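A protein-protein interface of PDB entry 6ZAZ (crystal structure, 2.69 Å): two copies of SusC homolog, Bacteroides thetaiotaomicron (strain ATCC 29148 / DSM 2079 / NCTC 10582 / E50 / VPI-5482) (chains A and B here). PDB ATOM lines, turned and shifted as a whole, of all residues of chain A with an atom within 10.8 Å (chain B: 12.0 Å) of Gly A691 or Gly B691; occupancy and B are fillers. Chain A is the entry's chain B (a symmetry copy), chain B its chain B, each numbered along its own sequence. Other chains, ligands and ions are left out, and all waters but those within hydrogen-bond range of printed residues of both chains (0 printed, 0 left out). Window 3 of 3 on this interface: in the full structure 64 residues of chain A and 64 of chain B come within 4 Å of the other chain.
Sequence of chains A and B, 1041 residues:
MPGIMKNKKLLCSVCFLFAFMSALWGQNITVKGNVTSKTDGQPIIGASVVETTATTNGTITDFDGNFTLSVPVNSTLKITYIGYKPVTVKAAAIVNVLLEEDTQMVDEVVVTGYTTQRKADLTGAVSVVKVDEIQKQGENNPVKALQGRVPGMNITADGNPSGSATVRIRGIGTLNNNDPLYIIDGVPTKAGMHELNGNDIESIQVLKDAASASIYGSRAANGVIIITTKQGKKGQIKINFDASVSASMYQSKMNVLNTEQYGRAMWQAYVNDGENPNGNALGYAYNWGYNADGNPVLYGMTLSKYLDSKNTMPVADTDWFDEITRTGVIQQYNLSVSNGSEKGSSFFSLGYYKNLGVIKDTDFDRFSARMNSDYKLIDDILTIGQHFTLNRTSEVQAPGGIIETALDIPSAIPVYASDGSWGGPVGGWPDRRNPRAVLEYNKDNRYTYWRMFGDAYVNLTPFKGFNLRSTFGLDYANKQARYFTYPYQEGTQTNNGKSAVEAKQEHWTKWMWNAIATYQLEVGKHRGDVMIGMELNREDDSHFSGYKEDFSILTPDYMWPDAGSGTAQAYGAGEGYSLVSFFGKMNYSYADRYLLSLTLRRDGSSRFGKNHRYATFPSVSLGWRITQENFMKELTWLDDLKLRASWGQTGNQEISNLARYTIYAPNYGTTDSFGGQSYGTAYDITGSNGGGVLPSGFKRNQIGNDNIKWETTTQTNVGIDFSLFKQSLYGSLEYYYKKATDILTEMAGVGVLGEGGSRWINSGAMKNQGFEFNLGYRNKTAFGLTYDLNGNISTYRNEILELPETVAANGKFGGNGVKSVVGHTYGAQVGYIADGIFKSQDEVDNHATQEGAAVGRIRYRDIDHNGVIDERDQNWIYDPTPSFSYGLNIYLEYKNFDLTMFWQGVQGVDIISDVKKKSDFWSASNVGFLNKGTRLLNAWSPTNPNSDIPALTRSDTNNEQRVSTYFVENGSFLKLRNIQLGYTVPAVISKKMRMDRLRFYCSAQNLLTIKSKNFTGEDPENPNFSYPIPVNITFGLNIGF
The side-chain hydroxyl (OH) of Tyr A668 is in hydrogen-bond range of the backbone NH (N) of Leu A694 (2.8 Å).
Printed residues of chain B within 4 Å of Thr A567: Val B693. No residue of chain B comes within 4 Å of Asn A689. No residue of chain B comes within 4 Å of Gly A690. Of chain B, only Gly B691 (3.6 Å) comes within 4 Å of Gly A691. No residue of chain B comes within 4 Å of Gly A692. Printed residues of chain B within 4 Å of Val A693: Ser B565 (3.7 Å), Gly B566 (3.9 Å) and Thr B567 (3.8 Å). Of the printed residues of chain A, Ser B565 touches Tyr A668 (3.5 Å) and Val A693 (3.7 Å). Printed residues of chain A within 4 Å of Gly B566: Val A693. Tyr B683 touches none of the printed residues of chain A. No residue of chain A comes within 4 Å of Gly B690. Of chain A, only Gly A691 (3.6 Å) comes within 4 Å of Gly B691. Printed residues of chain A within 4 Å of Val B693: Thr A567 (3.8 Å). The nearest residue of chain B that does not touch Gly A691 is Gly B692 (4.5 Å). The nearest residue of chain A that does not touch Gly B691 is Gly A692 (4.5 Å). The nearest printed residue of chain A that does not touch Ser B565 is Leu A694 (4.5 Å).
Thr A567 touches Val B693, and with the chains exchanged Val A693 touches Thr B567. Gly B691 touches its own counterpart, Gly A691. Positions printed for both chains: 567, 668, 683, 684, 685, 686, 687, 688, 689, 690, 691, 692, 693, 694 and 695.
Printed residues of chain B that touch a printed residue of chain A: Ser B565, Gly B566, Thr B567, Gly B691 and Val B693. Along chain B the printed residues that touch a printed residue of chain A span positions 565 to 693. Of the 15 printed residues of chain A, 4 touch a printed residue of chain B. Printed residues of chain A that touch a printed residue of chain B: Thr A567, Tyr A668, Gly A691 and Val A693. Among the printed residues, 6 pairs touch across the chains. Among the printed residues, no Asp or Glu carboxylate lies within 4 Å of a Lys or Arg side-chain nitrogen of the other chain.
Thr A567 touches Val B693. Tyr A668 touches Ser B565 (CE2 to O, 3.5 Å). CA of Gly A691 touches CA of Gly B691, at 3.6 Å. Ser B565 touches Val A693 (O to CG1, 3.7 Å). Gly B566 touches Val A693. CG2 of Val A693 touches OG1 of Thr B567, 3.8 Å away.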
ATOM      1  N   THR A 567      16.375 -11.771 -20.269  1.00  0.00           N
ATOM      2  CA  THR A 567      15.458 -12.877 -20.488  1.00  0.00           C
ATOM      3  C   THR A 567      16.201 -14.164 -20.838  1.00  0.00           C
ATOM      4  O   THR A 567      17.268 -14.155 -21.466  1.00  0.00           O
ATOM      5  CB  THR A 567      14.460 -12.546 -21.600  1.00  0.00           C
ATOM      6  OG1 THR A 567      14.133 -11.154 -21.567  1.00  0.00           O
ATOM      7  CG2 THR A 567      13.201 -13.330 -21.373  1.00  0.00           C
ATOM      8  N   TYR A 668       5.160 -22.437 -28.283  1.00  0.00           N
ATOM      9  CA  TYR A 668       4.804 -21.156 -27.677  1.00  0.00           C
ATOM     10  C   TYR A 668       5.402 -19.999 -28.458  1.00  0.00           C
ATOM     11  O   TYR A 668       4.793 -18.927 -28.557  1.00  0.00           O
ATOM     12  CB  TYR A 668       5.281 -21.138 -26.215  1.00  0.00           C
ATOM     13  CG  TYR A 668       4.930 -19.896 -25.408  1.00  0.00           C
ATOM     14  CD1 TYR A 668       5.672 -18.718 -25.514  1.00  0.00           C
ATOM     15  CD2 TYR A 668       3.872 -19.912 -24.508  1.00  0.00           C
ATOM     16  CE1 TYR A 668       5.345 -17.573 -24.764  1.00  0.00           C
ATOM     17  CE2 TYR A 668       3.544 -18.784 -23.754  1.00  0.00           C
ATOM     18  CZ  TYR A 668       4.285 -17.620 -23.880  1.00  0.00           C
ATOM     19  OH  TYR A 668       3.947 -16.515 -23.113  1.00  0.00           O
ATOM     20  N   TYR A 683      -0.724 -16.101 -27.361  1.00  0.00           N
ATOM     21  CA  TYR A 683      -1.441 -14.895 -27.765  1.00  0.00           C
ATOM     22  C   TYR A 683      -1.982 -14.176 -26.530  1.00  0.00           C
ATOM     23  O   TYR A 683      -2.503 -14.802 -25.600  1.00  0.00           O
ATOM     24  CB  TYR A 683      -2.585 -15.226 -28.747  1.00  0.00           C
ATOM     25  CG  TYR A 683      -3.284 -14.020 -29.383  1.00  0.00           C
ATOM     26  CD1 TYR A 683      -2.623 -13.192 -30.279  1.00  0.00           C
ATOM     27  CD2 TYR A 683      -4.610 -13.724 -29.084  1.00  0.00           C
ATOM     28  CE1 TYR A 683      -3.259 -12.101 -30.854  1.00  0.00           C
ATOM     29  CE2 TYR A 683      -5.253 -12.650 -29.666  1.00  0.00           C
ATOM     30  CZ  TYR A 683      -4.571 -11.838 -30.550  1.00  0.00           C
ATOM     31  OH  TYR A 683      -5.209 -10.759 -31.125  1.00  0.00           O
ATOM     32  N   ASP A 684      -1.868 -12.852 -26.547  1.00  0.00           N
ATOM     33  CA  ASP A 684      -2.412 -11.995 -25.486  1.00  0.00           C
ATOM     34  C   ASP A 684      -3.931 -11.882 -25.656  1.00  0.00           C
ATOM     35  O   ASP A 684      -4.488 -10.823 -25.956  1.00  0.00           O
ATOM     36  CB  ASP A 684      -1.722 -10.635 -25.528  1.00  0.00           C
ATOM     37  CG  ASP A 684      -2.261  -9.658 -24.516  1.00  0.00           C
ATOM     38  OD1 ASP A 684      -2.683 -10.096 -23.427  1.00  0.00           O
ATOM     39  OD2 ASP A 684      -2.266  -8.440 -24.819  1.00  0.00           O
ATOM     40  N   ILE A 685      -4.610 -13.020 -25.470  1.00  0.00           N
ATOM     41  CA  ILE A 685      -6.068 -13.058 -25.590  1.00  0.00           C
ATOM     42  C   ILE A 685      -6.736 -12.036 -24.686  1.00  0.00           C
ATOM     43  O   ILE A 685      -7.877 -11.635 -24.936  1.00  0.00           O
ATOM     44  CB  ILE A 685      -6.608 -14.476 -25.282  1.00  0.00           C
ATOM     45  CG1 ILE A 685      -8.078 -14.611 -25.676  1.00  0.00           C
ATOM     46  CG2 ILE A 685      -6.524 -14.754 -23.814  1.00  0.00           C
ATOM     47  CD1 ILE A 685      -8.342 -14.478 -27.145  1.00  0.00           C
ATOM     48  N   THR A 686      -6.052 -11.595 -23.637  1.00  0.00           N
ATOM     49  CA  THR A 686      -6.685 -10.711 -22.673  1.00  0.00           C
ATOM     50  C   THR A 686      -6.576  -9.254 -23.068  1.00  0.00           C
ATOM     51  O   THR A 686      -7.419  -8.461 -22.633  1.00  0.00           O
ATOM     52  CB  THR A 686      -6.083 -10.901 -21.277  1.00  0.00           C
ATOM     53  OG1 THR A 686      -4.676 -11.168 -21.391  1.00  0.00           O
ATOM     54  CG2 THR A 686      -6.776 -12.053 -20.548  1.00  0.00           C
ATOM     55  N   GLY A 687      -5.574  -8.895 -23.878  1.00  0.00           N
ATOM     56  CA  GLY A 687      -5.357  -7.514 -24.267  1.00  0.00           C
ATOM     57  C   GLY A 687      -4.575  -6.700 -23.261  1.00  0.00           C
ATOM     58  O   GLY A 687      -4.721  -5.470 -23.215  1.00  0.00           O
ATOM     59  N   SER A 688      -3.760  -7.357 -22.438  1.00  0.00           N
ATOM     60  CA  SER A 688      -2.974  -6.699 -21.403  1.00  0.00           C
ATOM     61  C   SER A 688      -1.703  -6.078 -21.941  1.00  0.00           C
ATOM     62  O   SER A 688      -1.150  -5.188 -21.293  1.00  0.00           O
ATOM     63  CB  SER A 688      -2.572  -7.709 -20.340  1.00  0.00           C
ATOM     64  OG  SER A 688      -1.588  -8.592 -20.867  1.00  0.00           O
ATOM     65  N   ASN A 689      -1.217  -6.584 -23.071  1.00  0.00           N
ATOM     66  CA  ASN A 689       0.005  -6.192 -23.768  1.00  0.00           C
ATOM     67  C   ASN A 689       1.168  -7.009 -23.238  1.00  0.00           C
ATOM     68  O   ASN A 689       2.324  -6.731 -23.568  1.00  0.00           O
ATOM     69  CB  ASN A 689       0.290  -4.693 -23.667  1.00  0.00           C
ATOM     70  CG  ASN A 689       0.861  -4.123 -24.968  1.00  0.00           C
ATOM     71  OD1 ASN A 689       0.920  -4.799 -25.986  1.00  0.00           O
ATOM     72  ND2 ASN A 689       1.270  -2.882 -24.932  1.00  0.00           N
ATOM     73  N   GLY A 690       0.862  -8.013 -22.409  1.00  0.00           N
ATOM     74  CA  GLY A 690       1.848  -8.957 -21.936  1.00  0.00           C
ATOM     75  C   GLY A 690       2.328  -8.709 -20.517  1.00  0.00           C
ATOM     76  O   GLY A 690       1.531  -8.365 -19.636  1.00  0.00           O
ATOM     77  N   GLY A 691       3.634  -8.870 -20.290  1.00  0.00           N
ATOM     78  CA  GLY A 691       4.185  -8.848 -18.947  1.00  0.00           C
ATOM     79  C   GLY A 691       3.793 -10.066 -18.127  1.00  0.00           C
ATOM     80  O   GLY A 691       3.033  -9.959 -17.164  1.00  0.00           O
ATOM     81  N   GLY A 692       4.304 -11.231 -18.495  1.00  0.00           N
ATOM     82  CA  GLY A 692       3.846 -12.486 -17.933  1.00  0.00           C
ATOM     83  C   GLY A 692       3.529 -13.507 -19.009  1.00  0.00           C
ATOM     84  O   GLY A 692       3.474 -13.208 -20.196  1.00  0.00           O
ATOM     85  N   VAL A 693       3.326 -14.739 -18.555  1.00  0.00           N
ATOM     86  CA  VAL A 693       3.114 -15.847 -19.470  1.00  0.00           C
ATOM     87  C   VAL A 693       1.765 -15.677 -20.153  1.00  0.00           C
ATOM     88  O   VAL A 693       0.748 -15.406 -19.497  1.00  0.00           O
ATOM     89  CB  VAL A 693       3.194 -17.178 -18.707  1.00  0.00           C
ATOM     90  CG1 VAL A 693       2.365 -18.265 -19.390  1.00  0.00           C
ATOM     91  CG2 VAL A 693       4.625 -17.620 -18.566  1.00  0.00           C
ATOM     92  N   LEU A 694       1.750 -15.831 -21.525  1.00  0.00           N
ATOM     93  CA  LEU A 694       0.496 -15.811 -22.267  1.00  0.00           C
ATOM     94  C   LEU A 694      -0.100 -17.218 -22.391  1.00  0.00           C
ATOM     95  O   LEU A 694       0.631 -18.222 -22.399  1.00  0.00           O
ATOM     96  CB  LEU A 694       0.722 -15.257 -23.663  1.00  0.00           C
ATOM     97  CG  LEU A 694       1.427 -13.934 -23.925  1.00  0.00           C
ATOM     98  CD1 LEU A 694       1.796 -13.905 -25.397  1.00  0.00           C
ATOM     99  CD2 LEU A 694       0.556 -12.710 -23.570  1.00  0.00           C
ATOM    100  N   PRO A 695      -1.419 -17.338 -22.515  1.00  0.00           N
ATOM    101  CA  PRO A 695      -1.998 -18.644 -22.890  1.00  0.00           C
ATOM    102  C   PRO A 695      -1.546 -19.071 -24.285  1.00  0.00           C
ATOM    103  O   PRO A 695      -1.335 -18.241 -25.172  1.00  0.00           O
ATOM    104  CB  PRO A 695      -3.517 -18.397 -22.831  1.00  0.00           C
ATOM    105  CG  PRO A 695      -3.691 -16.901 -22.782  1.00  0.00           C
ATOM    106  CD  PRO A 695      -2.452 -16.368 -22.117  1.00  0.00           C
ATOM    107  N   SER B 565       5.206 -24.357 -21.963  1.00  0.00           N
ATOM    108  CA  SER B 565       4.426 -23.170 -22.276  1.00  0.00           C
ATOM    109  C   SER B 565       4.557 -22.103 -21.200  1.00  0.00           C
ATOM    110  O   SER B 565       3.752 -21.170 -21.167  1.00  0.00           O
ATOM    111  CB  SER B 565       2.948 -23.539 -22.485  1.00  0.00           C
ATOM    112  OG  SER B 565       2.387 -24.256 -21.384  1.00  0.00           O
ATOM    113  N   GLY B 566       5.544 -22.225 -20.314  1.00  0.00           N
ATOM    114  CA  GLY B 566       5.719 -21.292 -19.227  1.00  0.00           C
ATOM    115  C   GLY B 566       7.108 -20.673 -19.210  1.00  0.00           C
ATOM    116  O   GLY B 566       7.784 -20.566 -20.226  1.00  0.00           O
ATOM    117  N   THR B 567       7.515 -20.256 -18.017  1.00  0.00           N
ATOM    118  CA  THR B 567       8.750 -19.503 -17.878  1.00  0.00           C
ATOM    119  C   THR B 567       9.976 -20.403 -18.016  1.00  0.00           C
ATOM    120  O   THR B 567       9.966 -21.586 -17.652  1.00  0.00           O
ATOM    121  CB  THR B 567       8.798 -18.781 -16.529  1.00  0.00           C
ATOM    122  OG1 THR B 567       7.486 -18.352 -16.155  1.00  0.00           O
ATOM    123  CG2 THR B 567       9.670 -17.566 -16.659  1.00  0.00           C
ATOM    124  N   TYR B 668      21.011 -12.124 -10.570  1.00  0.00           N
ATOM    125  CA  TYR B 668      19.686 -11.538 -10.759  1.00  0.00           C
ATOM    126  C   TYR B 668      18.659 -12.219  -9.871  1.00  0.00           C
ATOM    127  O   TYR B 668      17.721 -11.573  -9.387  1.00  0.00           O
ATOM    128  CB  TYR B 668      19.291 -11.647 -12.242  1.00  0.00           C
ATOM    129  CG  TYR B 668      17.959 -11.020 -12.630  1.00  0.00           C
ATOM    130  CD1 TYR B 668      16.747 -11.676 -12.406  1.00  0.00           C
ATOM    131  CD2 TYR B 668      17.915  -9.782 -13.256  1.00  0.00           C
ATOM    132  CE1 TYR B 668      15.518 -11.094 -12.771  1.00  0.00           C
ATOM    133  CE2 TYR B 668      16.702  -9.198 -13.627  1.00  0.00           C
ATOM    134  CZ  TYR B 668      15.508  -9.859 -13.389  1.00  0.00           C
ATOM    135  OH  TYR B 668      14.316  -9.265 -13.774  1.00  0.00           O
ATOM    136  N   ALA B 682      18.093  -8.164  -8.520  1.00  0.00           N
ATOM    137  CA  ALA B 682      17.000  -7.503  -9.216  1.00  0.00           C
ATOM    138  C   ALA B 682      16.062  -6.832  -8.215  1.00  0.00           C
ATOM    139  O   ALA B 682      15.888  -7.301  -7.084  1.00  0.00           O
ATOM    140  CB  ALA B 682      16.232  -8.511 -10.069  1.00  0.00           C
ATOM    141  N   TYR B 683      15.434  -5.736  -8.645  1.00  0.00           N
ATOM    142  CA  TYR B 683      14.447  -5.049  -7.817  1.00  0.00           C
ATOM    143  C   TYR B 683      13.553  -4.174  -8.694  1.00  0.00           C
ATOM    144  O   TYR B 683      14.024  -3.494  -9.613  1.00  0.00           O
ATOM    145  CB  TYR B 683      15.127  -4.203  -6.719  1.00  0.00           C
ATOM    146  CG  TYR B 683      14.186  -3.589  -5.677  1.00  0.00           C
ATOM    147  CD1 TYR B 683      13.495  -4.383  -4.772  1.00  0.00           C
ATOM    148  CD2 TYR B 683      14.005  -2.212  -5.601  1.00  0.00           C
ATOM    149  CE1 TYR B 683      12.645  -3.825  -3.828  1.00  0.00           C
ATOM    150  CE2 TYR B 683      13.175  -1.650  -4.653  1.00  0.00           C
ATOM    151  CZ  TYR B 683      12.493  -2.463  -3.768  1.00  0.00           C
ATOM    152  OH  TYR B 683      11.655  -1.903  -2.827  1.00  0.00           O
ATOM    153  N   ASP B 684      12.260  -4.191  -8.386  1.00  0.00           N
ATOM    154  CA  ASP B 684      11.271  -3.346  -9.066  1.00  0.00           C
ATOM    155  C   ASP B 684      11.393  -1.908  -8.548  1.00  0.00           C
ATOM    156  O   ASP B 684      10.505  -1.362  -7.889  1.00  0.00           O
ATOM    157  CB  ASP B 684       9.875  -3.922  -8.848  1.00  0.00           C
ATOM    158  CG  ASP B 684       8.779  -3.084  -9.454  1.00  0.00           C
ATOM    159  OD1 ASP B 684       9.022  -2.446 -10.498  1.00  0.00           O
ATOM    160  OD2 ASP B 684       7.667  -3.062  -8.873  1.00  0.00           O
ATOM    161  N   ILE B 685      12.542  -1.291  -8.850  1.00  0.00           N
ATOM    162  CA  ILE B 685      12.791   0.089  -8.430  1.00  0.00           C
ATOM    163  C   ILE B 685      11.692   1.029  -8.896  1.00  0.00           C
ATOM    164  O   ILE B 685      11.504   2.103  -8.315  1.00  0.00           O
ATOM    165  CB  ILE B 685      14.166   0.580  -8.947  1.00  0.00           C
ATOM    166  CG1 ILE B 685      14.570   1.898  -8.288  1.00  0.00           C
ATOM    167  CG2 ILE B 685      14.106   0.831 -10.421  1.00  0.00           C
ATOM    168  CD1 ILE B 685      14.793   1.810  -6.809  1.00  0.00           C
ATOM    169  N   THR B 686      10.951   0.652  -9.929  1.00  0.00           N
ATOM    170  CA  THR B 686       9.967   1.562 -10.493  1.00  0.00           C
ATOM    171  C   THR B 686       8.629   1.470  -9.792  1.00  0.00           C
ATOM    172  O   THR B 686       7.876   2.449  -9.830  1.00  0.00           O
ATOM    173  CB  THR B 686       9.772   1.301 -11.990  1.00  0.00           C
ATOM    174  OG1 THR B 686       9.874  -0.108 -12.251  1.00  0.00           O
ATOM    175  CG2 THR B 686      10.818   2.061 -12.806  1.00  0.00           C
ATOM    176  N   GLY B 687       8.328   0.332  -9.156  1.00  0.00           N
ATOM    177  CA  GLY B 687       7.048   0.131  -8.503  1.00  0.00           C
ATOM    178  C   GLY B 687       5.942  -0.322  -9.429  1.00  0.00           C
ATOM    179  O   GLY B 687       4.761  -0.078  -9.145  1.00  0.00           O
ATOM    180  N   SER B 688       6.295  -0.962 -10.541  1.00  0.00           N
ATOM    181  CA  SER B 688       5.333  -1.426 -11.533  1.00  0.00           C
ATOM    182  C   SER B 688       4.685  -2.739 -11.151  1.00  0.00           C
ATOM    183  O   SER B 688       3.614  -3.052 -11.669  1.00  0.00           O
ATOM    184  CB  SER B 688       6.029  -1.634 -12.869  1.00  0.00           C
ATOM    185  OG  SER B 688       6.872  -2.779 -12.795  1.00  0.00           O
ATOM    186  N   ASN B 689       5.357  -3.518 -10.308  1.00  0.00           N
ATOM    187  CA  ASN B 689       4.973  -4.839  -9.818  1.00  0.00           C
ATOM    188  C   ASN B 689       5.500  -5.898 -10.769  1.00  0.00           C
ATOM    189  O   ASN B 689       5.154  -7.076 -10.639  1.00  0.00           O
ATOM    190  CB  ASN B 689       3.463  -4.980  -9.616  1.00  0.00           C
ATOM    191  CG  ASN B 689       3.121  -5.803  -8.371  1.00  0.00           C
ATOM    192  OD1 ASN B 689       3.988  -6.155  -7.583  1.00  0.00           O
ATOM    193  ND2 ASN B 689       1.860  -6.097  -8.195  1.00  0.00           N
ATOM    194  N   GLY B 690       6.332  -5.478 -11.728  1.00  0.00           N
ATOM    195  CA  GLY B 690       7.015  -6.388 -12.617  1.00  0.00           C
ATOM    196  C   GLY B 690       6.406  -6.493 -14.003  1.00  0.00           C
ATOM    197  O   GLY B 690       5.985  -5.485 -14.582  1.00  0.00           O
ATOM    198  N   GLY B 691       6.346  -7.714 -14.539  1.00  0.00           N
ATOM    199  CA  GLY B 691       5.964  -7.923 -15.924  1.00  0.00           C
ATOM    200  C   GLY B 691       7.014  -7.437 -16.908  1.00  0.00           C
ATOM    201  O   GLY B 691       6.799  -6.463 -17.629  1.00  0.00           O
ATOM    202  N   GLY B 692       8.156  -8.107 -16.952  1.00  0.00           N
ATOM    203  CA  GLY B 692       9.307  -7.622 -17.686  1.00  0.00           C
ATOM    204  C   GLY B 692      10.569  -7.650 -16.845  1.00  0.00           C
ATOM    205  O   GLY B 692      10.545  -7.860 -15.636  1.00  0.00           O
ATOM    206  N   VAL B 693      11.689  -7.436 -17.527  1.00  0.00           N
ATOM    207  CA  VAL B 693      12.987  -7.533 -16.881  1.00  0.00           C
ATOM    208  C   VAL B 693      13.144  -6.379 -15.901  1.00  0.00           C
ATOM    209  O   VAL B 693      12.869  -5.217 -16.237  1.00  0.00           O
ATOM    210  CB  VAL B 693      14.100  -7.527 -17.940  1.00  0.00           C
ATOM    211  CG1 VAL B 693      15.406  -6.969 -17.375  1.00  0.00           C
ATOM    212  CG2 VAL B 693      14.314  -8.910 -18.489  1.00  0.00           C
ATOM    213  N   LEU B 694      13.591  -6.706 -14.637  1.00  0.00           N
ATOM    214  CA  LEU B 694      13.893  -5.670 -13.659  1.00  0.00           C
ATOM    215  C   LEU B 694      15.358  -5.227 -13.751  1.00  0.00           C
ATOM    216  O   LEU B 694      16.238  -6.011 -14.143  1.00  0.00           O
ATOM    217  CB  LEU B 694      13.632  -6.183 -12.253  1.00  0.00           C
ATOM    218  CG  LEU B 694      12.317  -6.830 -11.841  1.00  0.00           C
ATOM    219  CD1 LEU B 694      12.560  -7.539 -10.521  1.00  0.00           C
ATOM    220  CD2 LEU B 694      11.168  -5.810 -11.693  1.00  0.00           C
ATOM    221  N   PRO B 695      15.672  -3.989 -13.376  1.00  0.00           N
ATOM    222  CA  PRO B 695      17.090  -3.616 -13.210  1.00  0.00           C
ATOM    223  C   PRO B 695      17.748  -4.422 -12.091  1.00  0.00           C
ATOM    224  O   PRO B 695      17.110  -4.777 -11.098  1.00  0.00           O
ATOM    225  CB  PRO B 695      17.034  -2.114 -12.877  1.00  0.00           C
ATOM    226  CG  PRO B 695      15.597  -1.822 -12.527  1.00  0.00           C
ATOM    227  CD  PRO B 695      14.779  -2.822 -13.296  1.00  0.00           C
